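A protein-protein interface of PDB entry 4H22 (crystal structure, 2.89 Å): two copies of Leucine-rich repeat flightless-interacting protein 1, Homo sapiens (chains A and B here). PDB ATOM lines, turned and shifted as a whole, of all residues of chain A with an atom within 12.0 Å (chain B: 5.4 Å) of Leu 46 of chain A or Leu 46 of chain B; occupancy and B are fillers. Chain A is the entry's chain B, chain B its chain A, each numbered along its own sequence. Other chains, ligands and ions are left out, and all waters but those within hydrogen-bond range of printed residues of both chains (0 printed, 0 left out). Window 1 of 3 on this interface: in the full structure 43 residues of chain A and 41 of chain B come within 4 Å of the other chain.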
ATOM      1  N   ASP A  37      22.431  -2.751  18.414  1.00  0.00           N
ATOM      2  CA  ASP A  37      21.427  -1.817  17.912  1.00  0.00           C
ATOM      3  C   ASP A  37      21.999  -0.863  16.882  1.00  0.00           C
ATOM      4  O   ASP A  37      21.442  -0.706  15.788  1.00  0.00           O
ATOM      5  CB  ASP A  37      20.839  -1.014  19.058  1.00  0.00           C
ATOM      6  CG  ASP A  37      19.634  -1.676  19.663  1.00  0.00           C
ATOM      7  OD1 ASP A  37      19.452  -2.904  19.463  1.00  0.00           O
ATOM      8  OD2 ASP A  37      18.861  -0.961  20.339  1.00  0.00           O
ATOM      9  N   MET A  38      23.118  -0.234  17.245  1.00  0.00           N
ATOM     10  CA  MET A  38      23.856   0.628  16.332  1.00  0.00           C
ATOM     11  C   MET A  38      24.144  -0.113  15.038  1.00  0.00           C
ATOM     12  O   MET A  38      23.919   0.421  13.955  1.00  0.00           O
ATOM     13  CB  MET A  38      25.146   1.128  16.979  1.00  0.00           C
ATOM     14  CG  MET A  38      24.889   2.142  18.093  1.00  0.00           C
ATOM     15  SD  MET A  38      26.340   2.713  19.018  1.00  0.00           S
ATOM     16  CE  MET A  38      27.415   3.322  17.706  1.00  0.00           C
ATOM     17  N   LEU A  39      24.588  -1.361  15.152  1.00  0.00           N
ATOM     18  CA  LEU A  39      24.924  -2.125  13.970  1.00  0.00           C
ATOM     19  C   LEU A  39      23.746  -2.187  13.026  1.00  0.00           C
ATOM     20  O   LEU A  39      23.885  -1.883  11.832  1.00  0.00           O
ATOM     21  CB  LEU A  39      25.402  -3.533  14.307  1.00  0.00           C
ATOM     22  CG  LEU A  39      25.883  -4.269  13.053  1.00  0.00           C
ATOM     23  CD1 LEU A  39      27.304  -3.862  12.687  1.00  0.00           C
ATOM     24  CD2 LEU A  39      25.797  -5.763  13.255  1.00  0.00           C
ATOM     25  N   LEU A  40      22.585  -2.554  13.558  1.00  0.00           N
ATOM     26  CA  LEU A  40      21.392  -2.668  12.722  1.00  0.00           C
ATOM     27  C   LEU A  40      20.911  -1.307  12.201  1.00  0.00           C
ATOM     28  O   LEU A  40      20.488  -1.196  11.038  1.00  0.00           O
ATOM     29  CB  LEU A  40      20.275  -3.412  13.458  1.00  0.00           C
ATOM     30  CG  LEU A  40      20.605  -4.839  13.917  1.00  0.00           C
ATOM     31  CD1 LEU A  40      19.497  -5.389  14.804  1.00  0.00           C
ATOM     32  CD2 LEU A  40      20.876  -5.776  12.741  1.00  0.00           C
ATOM     33  N   GLU A  41      21.004  -0.281  13.056  1.00  0.00           N
ATOM     34  CA  GLU A  41      20.666   1.095  12.675  1.00  0.00           C
ATOM     35  C   GLU A  41      21.466   1.511  11.445  1.00  0.00           C
ATOM     36  O   GLU A  41      20.903   2.011  10.465  1.00  0.00           O
ATOM     37  CB  GLU A  41      20.890   2.073  13.844  1.00  0.00           C
ATOM     38  CG  GLU A  41      20.885   3.563  13.481  1.00  0.00           C
ATOM     39  CD  GLU A  41      19.562   4.047  12.895  1.00  0.00           C
ATOM     40  OE1 GLU A  41      18.505   3.521  13.298  1.00  0.00           O
ATOM     41  OE2 GLU A  41      19.574   4.957  12.034  1.00  0.00           O
ATOM     42  N   LEU A  42      22.769   1.264  11.485  1.00  0.00           N
ATOM     43  CA  LEU A  42      23.621   1.531  10.331  1.00  0.00           C
ATOM     44  C   LEU A  42      23.235   0.711   9.114  1.00  0.00           C
ATOM     45  O   LEU A  42      23.130   1.263   8.019  1.00  0.00           O
ATOM     46  CB  LEU A  42      25.101   1.347  10.663  1.00  0.00           C
ATOM     47  CG  LEU A  42      25.686   2.379  11.637  1.00  0.00           C
ATOM     48  CD1 LEU A  42      27.184   2.156  11.753  1.00  0.00           C
ATOM     49  CD2 LEU A  42      25.380   3.825  11.227  1.00  0.00           C
ATOM     50  N   GLU A  43      22.980  -0.586   9.298  1.00  0.00           N
ATOM     51  CA  GLU A  43      22.488  -1.395   8.189  1.00  0.00           C
ATOM     52  C   GLU A  43      21.303  -0.695   7.514  1.00  0.00           C
ATOM     53  O   GLU A  43      21.264  -0.581   6.284  1.00  0.00           O
ATOM     54  CB  GLU A  43      22.097  -2.796   8.642  1.00  0.00           C
ATOM     55  CG  GLU A  43      21.604  -3.707   7.515  1.00  0.00           C
ATOM     56  CD  GLU A  43      20.140  -3.494   7.137  1.00  0.00           C
ATOM     57  OE1 GLU A  43      19.316  -3.144   8.015  1.00  0.00           O
ATOM     58  OE2 GLU A  43      19.803  -3.680   5.946  1.00  0.00           O
ATOM     59  N   GLU A  44      20.349  -0.220   8.312  1.00  0.00           N
ATOM     60  CA  GLU A  44      19.210   0.495   7.758  1.00  0.00           C
ATOM     61  C   GLU A  44      19.685   1.666   6.903  1.00  0.00           C
ATOM     62  O   GLU A  44      19.329   1.770   5.724  1.00  0.00           O
ATOM     63  CB  GLU A  44      18.251   0.961   8.856  1.00  0.00           C
ATOM     64  CG  GLU A  44      17.440  -0.171   9.470  1.00  0.00           C
ATOM     65  CD  GLU A  44      16.528   0.274  10.604  1.00  0.00           C
ATOM     66  OE1 GLU A  44      16.800   1.319  11.239  1.00  0.00           O
ATOM     67  OE2 GLU A  44      15.538  -0.441  10.877  1.00  0.00           O
ATOM     68  N   GLN A  45      20.528   2.516   7.485  1.00  0.00           N
ATOM     69  CA  GLN A  45      21.066   3.666   6.766  1.00  0.00           C
ATOM     70  C   GLN A  45      21.789   3.272   5.475  1.00  0.00           C
ATOM     71  O   GLN A  45      21.547   3.849   4.412  1.00  0.00           O
ATOM     72  CB  GLN A  45      21.984   4.474   7.672  1.00  0.00           C
ATOM     73  CG  GLN A  45      21.231   5.275   8.718  1.00  0.00           C
ATOM     74  CD  GLN A  45      22.143   6.086   9.616  1.00  0.00           C
ATOM     75  OE1 GLN A  45      23.142   6.650   9.171  1.00  0.00           O
ATOM     76  NE2 GLN A  45      21.789   6.161  10.888  1.00  0.00           N
ATOM     77  N   LEU A  46      22.660   2.275   5.562  1.00  0.00           N
ATOM     78  CA  LEU A  46      23.377   1.829   4.386  1.00  0.00           C
ATOM     79  C   LEU A  46      22.407   1.408   3.295  1.00  0.00           C
ATOM     80  O   LEU A  46      22.641   1.697   2.122  1.00  0.00           O
ATOM     81  CB  LEU A  46      24.359   0.702   4.706  1.00  0.00           C
ATOM     82  CG  LEU A  46      25.166   0.196   3.502  1.00  0.00           C
ATOM     83  CD1 LEU A  46      25.951   1.341   2.882  1.00  0.00           C
ATOM     84  CD2 LEU A  46      26.096  -0.969   3.827  1.00  0.00           C
ATOM     85  N   ALA A  47      21.314   0.746   3.677  1.00  0.00           N
ATOM     86  CA  ALA A  47      20.353   0.249   2.691  1.00  0.00           C
ATOM     87  C   ALA A  47      19.600   1.404   2.054  1.00  0.00           C
ATOM     88  O   ALA A  47      19.298   1.377   0.856  1.00  0.00           O
ATOM     89  CB  ALA A  47      19.389  -0.745   3.318  1.00  0.00           C
ATOM     90  N   GLU A  48      19.309   2.414   2.872  1.00  0.00           N
ATOM     91  CA  GLU A  48      18.728   3.670   2.418  1.00  0.00           C
ATOM     92  C   GLU A  48      19.641   4.309   1.362  1.00  0.00           C
ATOM     93  O   GLU A  48      19.195   4.673   0.264  1.00  0.00           O
ATOM     94  CB  GLU A  48      18.559   4.616   3.610  1.00  0.00           C
ATOM     95  CG  GLU A  48      17.650   5.804   3.351  1.00  0.00           C
ATOM     96  CD  GLU A  48      16.192   5.475   3.601  1.00  0.00           C
ATOM     97  OE1 GLU A  48      15.852   5.166   4.765  1.00  0.00           O
ATOM     98  OE2 GLU A  48      15.388   5.527   2.640  1.00  0.00           O
ATOM     99  N   SER A  49      20.922   4.416   1.703  1.00  0.00           N
ATOM    100  CA  SER A  49      21.897   5.052   0.850  1.00  0.00           C
ATOM    101  C   SER A  49      22.065   4.306  -0.467  1.00  0.00           C
ATOM    102  O   SER A  49      22.165   4.935  -1.525  1.00  0.00           O
ATOM    103  CB  SER A  49      23.232   5.141   1.575  1.00  0.00           C
ATOM    104  OG  SER A  49      24.180   5.862   0.804  1.00  0.00           O
ATOM    105  N   ARG A  50      22.084   2.973  -0.415  1.00  0.00           N
ATOM    106  CA  ARG A  50      22.224   2.179  -1.638  1.00  0.00           C
ATOM    107  C   ARG A  50      21.046   2.363  -2.595  1.00  0.00           C
ATOM    108  O   ARG A  50      21.214   2.304  -3.820  1.00  0.00           O
ATOM    109  CB  ARG A  50      22.464   0.705  -1.338  1.00  0.00           C
ATOM    110  CG  ARG A  50      23.894   0.408  -0.922  1.00  0.00           C
ATOM    111  CD  ARG A  50      24.379  -0.940  -1.456  1.00  0.00           C
ATOM    112  NE  ARG A  50      25.223  -1.641  -0.478  1.00  0.00           N
ATOM    113  CZ  ARG A  50      26.522  -1.397  -0.261  1.00  0.00           C
ATOM    114  NH1 ARG A  50      27.169  -0.466  -0.958  1.00  0.00           N
ATOM    115  NH2 ARG A  50      27.181  -2.092   0.665  1.00  0.00           N
ATOM    116  N   ARG A  51      19.863   2.612  -2.035  1.00  0.00           N
ATOM    117  CA  ARG A  51      18.683   2.857  -2.844  1.00  0.00           C
ATOM    118  C   ARG A  51      18.843   4.164  -3.606  1.00  0.00           C
ATOM    119  O   ARG A  51      18.675   4.197  -4.828  1.00  0.00           O
ATOM    120  CB  ARG A  51      17.436   2.892  -1.972  1.00  0.00           C
ATOM    121  CG  ARG A  51      16.160   3.052  -2.772  1.00  0.00           C
ATOM    122  CD  ARG A  51      14.935   3.052  -1.881  1.00  0.00           C
ATOM    123  NE  ARG A  51      13.738   3.285  -2.678  1.00  0.00           N
ATOM    124  CZ  ARG A  51      12.503   3.312  -2.198  1.00  0.00           C
ATOM    125  NH1 ARG A  51      12.273   3.113  -0.905  1.00  0.00           N
ATOM    126  NH2 ARG A  51      11.494   3.546  -3.020  1.00  0.00           N
ATOM    127  N   GLN A  52      19.182   5.225  -2.873  1.00  0.00           N
ATOM    128  CA  GLN A  52      19.462   6.541  -3.450  1.00  0.00           C
ATOM    129  C   GLN A  52      20.431   6.443  -4.612  1.00  0.00           C
ATOM    130  O   GLN A  52      20.084   6.772  -5.752  1.00  0.00           O
ATOM    131  CB  GLN A  52      20.028   7.491  -2.401  1.00  0.00           C
ATOM    132  CG  GLN A  52      18.969   8.166  -1.548  1.00  0.00           C
ATOM    133  CD  GLN A  52      19.523   8.699  -0.240  1.00  0.00           C
ATOM    134  OE1 GLN A  52      20.729   8.612   0.030  1.00  0.00           O
ATOM    135  NE2 GLN A  52      18.642   9.246   0.590  1.00  0.00           N
ATOM    136  N   TYR A  53      21.637   5.962  -4.335  1.00  0.00           N
ATOM    137  CA  TYR A  53      22.612   5.801  -5.395  1.00  0.00           C
ATOM    138  C   TYR A  53      22.022   5.066  -6.599  1.00  0.00           C
ATOM    139  O   TYR A  53      22.188   5.507  -7.736  1.00  0.00           O
ATOM    140  CB  TYR A  53      23.867   5.083  -4.912  1.00  0.00           C
ATOM    141  CG  TYR A  53      24.791   4.772  -6.063  1.00  0.00           C
ATOM    142  CD1 TYR A  53      25.747   5.700  -6.478  1.00  0.00           C
ATOM    143  CD2 TYR A  53      24.677   3.570  -6.773  1.00  0.00           C
ATOM    144  CE1 TYR A  53      26.581   5.430  -7.553  1.00  0.00           C
ATOM    145  CE2 TYR A  53      25.500   3.297  -7.849  1.00  0.00           C
ATOM    146  CZ  TYR A  53      26.450   4.229  -8.236  1.00  0.00           C
ATOM    147  OH  TYR A  53      27.276   3.972  -9.304  1.00  0.00           O
ATOM    148  N   GLU A  54      21.339   3.950  -6.347  1.00  0.00           N
ATOM    149  CA  GLU A  54      20.813   3.118  -7.423  1.00  0.00           C
ATOM    150  C   GLU A  54      19.793   3.883  -8.260  1.00  0.00           C
ATOM    151  O   GLU A  54      19.843   3.877  -9.491  1.00  0.00           O
ATOM    152  CB  GLU A  54      20.194   1.846  -6.854  1.00  0.00           C
ATOM    153  CG  GLU A  54      20.602   0.584  -7.596  1.00  0.00           C
ATOM    154  CD  GLU A  54      22.111   0.434  -7.696  1.00  0.00           C
ATOM    155  OE1 GLU A  54      22.630   0.458  -8.830  1.00  0.00           O
ATOM    156  OE2 GLU A  54      22.784   0.315  -6.648  1.00  0.00           O
ATOM    157  N   GLU A  55      18.894   4.577  -7.577  1.00  0.00           N
ATOM    158  CA  GLU A  55      17.845   5.323  -8.241  1.00  0.00           C
ATOM    159  C   GLU A  55      18.351   6.559  -8.994  1.00  0.00           C
ATOM    160  O   GLU A  55      17.844   6.858 -10.078  1.00  0.00           O
ATOM    161  CB  GLU A  55      16.729   5.645  -7.252  1.00  0.00           C
ATOM    162  CG  GLU A  55      15.952   4.392  -6.878  1.00  0.00           C
ATOM    163  CD  GLU A  55      14.902   4.610  -5.809  1.00  0.00           C
ATOM    164  OE1 GLU A  55      14.804   5.737  -5.272  1.00  0.00           O
ATOM    165  OE2 GLU A  55      14.173   3.637  -5.506  1.00  0.00           O
ATOM    166  N   LEU B  42      31.668  -0.436   8.858  1.00  0.00           N
ATOM    167  CA  LEU B  42      30.369  -0.111   8.301  1.00  0.00           C
ATOM    168  C   LEU B  42      30.211   1.354   7.943  1.00  0.00           C
ATOM    169  O   LEU B  42      29.762   1.662   6.837  1.00  0.00           O
ATOM    170  CB  LEU B  42      29.242  -0.545   9.228  1.00  0.00           C
ATOM    171  CG  LEU B  42      28.063  -1.067   8.421  1.00  0.00           C
ATOM    172  CD1 LEU B  42      28.469  -2.374   7.749  1.00  0.00           C
ATOM    173  CD2 LEU B  42      26.853  -1.258   9.314  1.00  0.00           C
ATOM    174  N   GLU B  43      30.561   2.258   8.857  1.00  0.00           N
ATOM    175  CA  GLU B  43      30.486   3.678   8.521  1.00  0.00           C
ATOM    176  C   GLU B  43      31.459   4.066   7.424  1.00  0.00           C
ATOM    177  O   GLU B  43      31.192   4.993   6.661  1.00  0.00           O
ATOM    178  CB  GLU B  43      30.596   4.605   9.725  1.00  0.00           C
ATOM    179  CG  GLU B  43      31.297   4.043  10.932  1.00  0.00           C
ATOM    180  CD  GLU B  43      30.708   4.592  12.212  1.00  0.00           C
ATOM    181  OE1 GLU B  43      29.567   5.114  12.160  1.00  0.00           O
ATOM    182  OE2 GLU B  43      31.385   4.497  13.263  1.00  0.00           O
ATOM    183  N   GLU B  44      32.558   3.330   7.319  1.00  0.00           N
ATOM    184  CA  GLU B  44      33.397   3.407   6.136  1.00  0.00           C
ATOM    185  C   GLU B  44      32.543   3.205   4.873  1.00  0.00           C
ATOM    186  O   GLU B  44      32.538   4.056   3.985  1.00  0.00           O
ATOM    187  CB  GLU B  44      34.527   2.378   6.216  1.00  0.00           C
ATOM    188  CG  GLU B  44      35.766   2.719   5.397  1.00  0.00           C
ATOM    189  CD  GLU B  44      37.030   2.086   5.961  1.00  0.00           C
ATOM    190  OE1 GLU B  44      37.632   1.221   5.275  1.00  0.00           O
ATOM    191  OE2 GLU B  44      37.421   2.444   7.096  1.00  0.00           O
ATOM    192  N   GLN B  45      31.795   2.101   4.826  1.00  0.00           N
ATOM    193  CA  GLN B  45      30.955   1.761   3.674  1.00  0.00           C
ATOM    194  C   GLN B  45      29.850   2.778   3.456  1.00  0.00           C
ATOM    195  O   GLN B  45      29.674   3.285   2.343  1.00  0.00           O
ATOM    196  CB  GLN B  45      30.301   0.402   3.857  1.00  0.00           C
ATOM    197  CG  GLN B  45      31.253  -0.765   3.965  1.00  0.00           C
ATOM    198  CD  GLN B  45      30.538  -2.082   3.770  1.00  0.00           C
ATOM    199  OE1 GLN B  45      29.440  -2.128   3.207  1.00  0.00           O
ATOM    200  NE2 GLN B  45      31.159  -3.166   4.224  1.00  0.00           N
ATOM    201  N   LEU B  46      29.091   3.044   4.520  1.00  0.00           N
ATOM    202  CA  LEU B  46      28.020   4.026   4.480  1.00  0.00           C
ATOM    203  C   LEU B  46      28.551   5.317   3.883  1.00  0.00           C
ATOM    204  O   LEU B  46      27.994   5.824   2.915  1.00  0.00           O
ATOM    205  CB  LEU B  46      27.457   4.270   5.881  1.00  0.00           C
ATOM    206  CG  LEU B  46      26.361   5.327   6.068  1.00  0.00           C
ATOM    207  CD1 LEU B  46      25.159   5.093   5.170  1.00  0.00           C
ATOM    208  CD2 LEU B  46      25.909   5.360   7.517  1.00  0.00           C
ATOM    209  N   ALA B  47      29.653   5.818   4.439  1.00  0.00           N
ATOM    210  CA  ALA B  47      30.242   7.071   3.980  1.00  0.00           C
ATOM    211  C   ALA B  47      30.570   7.013   2.492  1.00  0.00           C
ATOM    212  O   ALA B  47      30.197   7.908   1.738  1.00  0.00           O
ATOM    213  CB  ALA B  47      31.475   7.423   4.799  1.00  0.00           C
ATOM    214  N   GLU B  48      31.245   5.945   2.076  1.00  0.00           N
ATOM    215  CA  GLU B  48      31.562   5.744   0.672  1.00  0.00           C
ATOM    216  C   GLU B  48      30.300   5.859  -0.178  1.00  0.00           C
ATOM    217  O   GLU B  48      30.225   6.710  -1.057  1.00  0.00           O
ATOM    218  CB  GLU B  48      32.249   4.394   0.458  1.00  0.00           C
ATOM    219  CG  GLU B  48      32.524   4.030  -0.997  1.00  0.00           C
ATOM    220  CD  GLU B  48      33.591   4.892  -1.664  1.00  0.00           C
ATOM    221  OE1 GLU B  48      34.344   5.602  -0.962  1.00  0.00           O
ATOM    222  OE2 GLU B  48      33.684   4.851  -2.908  1.00  0.00           O
ATOM    223  N   SER B  49      29.308   5.019   0.111  1.00  0.00           N
ATOM    224  CA  SER B  49      28.016   5.060  -0.566  1.00  0.00           C
ATOM    225  C   SER B  49      27.460   6.488  -0.649  1.00  0.00           C
ATOM    226  O   SER B  49      27.103   6.956  -1.730  1.00  0.00           O
ATOM    227  CB  SER B  49      27.023   4.134   0.144  1.00  0.00           C
ATOM    228  OG  SER B  49      25.797   4.021  -0.568  1.00  0.00           O
ATOM    229  N   ARG B  50      27.412   7.189   0.479  1.00  0.00           N
ATOM    230  CA  ARG B  50      26.936   8.567   0.489  1.00  0.00           C
ATOM    231  C   ARG B  50      27.749   9.471  -0.432  1.00  0.00           C
ATOM    232  O   ARG B  50      27.194  10.318  -1.127  1.00  0.00           O
ATOM    233  CB  ARG B  50      26.914   9.120   1.908  1.00  0.00           C
ATOM    234  CG  ARG B  50      25.681   8.686   2.679  1.00  0.00           C
ATOM    235  CD  ARG B  50      25.812   8.959   4.164  1.00  0.00           C
ATOM    236  NE  ARG B  50      24.568   8.660   4.877  1.00  0.00           N
ATOM    237  CZ  ARG B  50      24.463   8.524   6.201  1.00  0.00           C
ATOM    238  NH1 ARG B  50      25.529   8.661   6.984  1.00  0.00           N
ATOM    239  NH2 ARG B  50      23.285   8.242   6.747  1.00  0.00           N
ATOM    240  N   ARG B  51      29.061   9.267  -0.448  1.00  0.00           N
ATOM    241  CA  ARG B  51      29.946   9.987  -1.346  1.00  0.00           C
ATOM    242  C   ARG B  51      29.643   9.634  -2.817  1.00  0.00           C
ATOM    243  O   ARG B  51      29.585  10.520  -3.674  1.00  0.00           O
ATOM    244  CB  ARG B  51      31.400   9.687  -0.974  1.00  0.00           C
ATOM    245  CG  ARG B  51      32.436  10.568  -1.653  1.00  0.00           C
ATOM    246  CD  ARG B  51      33.781   9.860  -1.771  1.00  0.00           C
ATOM    247  NE  ARG B  51      33.674   8.569  -2.464  1.00  0.00           N
ATOM    248  CZ  ARG B  51      33.774   8.395  -3.782  1.00  0.00           C
ATOM    249  NH1 ARG B  51      33.993   9.426  -4.592  1.00  0.00           N
ATOM    250  NH2 ARG B  51      33.649   7.178  -4.293  1.00  0.00           N
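The side-chain amide oxygen of Gln 45 of chain B lies within hydrogen-bond range of the guanidinium group of Arg 50 of chain A, at 3.4 Å. The side-chain hydroxyl of Ser 49 of chain A sits at hydrogen-bond distance from the side-chain hydroxyl of Ser 49 of chain B (2.8 Å). NH2 of Arg 50 of chain B is in hydrogen-bond range of OE1 of Gln 45 of chain A (2.9 Å).
The side-chain carboxylate (OE2) of Glu 41 of chain A is in hydrogen-bond range of the side-chain amide nitrogen (NE2) of Gln 45 of chain A (2.8 Å).
Among the printed residues, merely in contact across the chains: Leu 42 of chain A with Leu 42 of chain B (3.4 Å), Gln 45 of chain A with Leu 46 of chain B (3.5 Å), Ser 49 of chain A with Arg 50 of chain B (3.5 Å), Leu 46 of chain A with Gln 45 of chain B (3.6 Å), Leu 46 of chain A with Leu 46 of chain B (3.7 Å), Leu 42 of chain A with Glu 43 of chain B (3.8 Å), Arg 50 of chain A with Ser 49 of chain B (3.9 Å), Glu 43 of chain A with Leu 42 of chain B (3.9 Å) and Leu 39 of chain A with Leu 42 of chain B (3.9 Å).
Of chain B, only Gln 45 (3.6 Å) and Leu 46 (3.7 Å) come within 4 Å of Leu 46 of chain A. Leu 46 of chain B touches just these residues of chain A: Gln 45 (3.5 Å) and Leu 46 (3.7 Å). Leu 42 of chain B touches three residues of chain A. No residue of chain A comes within 4 Å of Ala 47 of chain B. Of the printed residues of chain A, Ser 49 of chain B touches Ser 49 (2.8 Å) and Arg 50 (3.9 Å). Of the printed residues of chain A, Arg 50 of chain B touches Gln 45 and Ser 49. Printed residues of chain B within 4 Å of Gln 45 of chain A: Leu 46 (3.5 Å) and Arg 50 (2.9 Å). Of the printed residues of chain B, Ser 49 of chain A touches Ser 49 (2.8 Å) and Arg 50 (3.5 Å). Printed residues of chain B within 4 Å of Leu 39 of chain A: Leu 42 (3.9 Å). Of the printed residues of chain B, Leu 42 of chain A touches Leu 42 (3.4 Å) and Glu 43 (3.8 Å). Glu 44 of chain B touches none of the printed residues of chain A. The nearest printed residue of chain A that does not touch Leu 46 of chain B is Leu 42 of chain A (4.05 Å).
Printed residues of chain B that touch a printed residue of chain A: Leu 42, Glu 43, Gln 45, Leu 46, Ser 49 and Arg 50. Hydrophobic or aromatic side chains of chain B within 4 Å of the printed part of chain A: Leu 42 and Leu 46. Among the printed residues, 12 pairs touch across the chains.
Leu 42 of chain A touches Glu 43 of chain B, and with the chains exchanged Glu 43 of chain A touches Leu 42 of chain B. Gln 45 of chain A touches Arg 50 of chain B, and with the chains exchanged Arg 50 of chain A touches Gln 45 of chain B. Ser 49 of chain B touches its own counterpart, Ser 49 of chain A. Ser 49 of chain A touches Arg 50 of chain B, and with the chains exchanged Arg 50 of chain A touches Ser 49 of chain B. 10 positions are printed for both chains. Of the 12 pairs that touch across the chains among the printed residues, 11 have their exchanged pair printed and touching as well.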
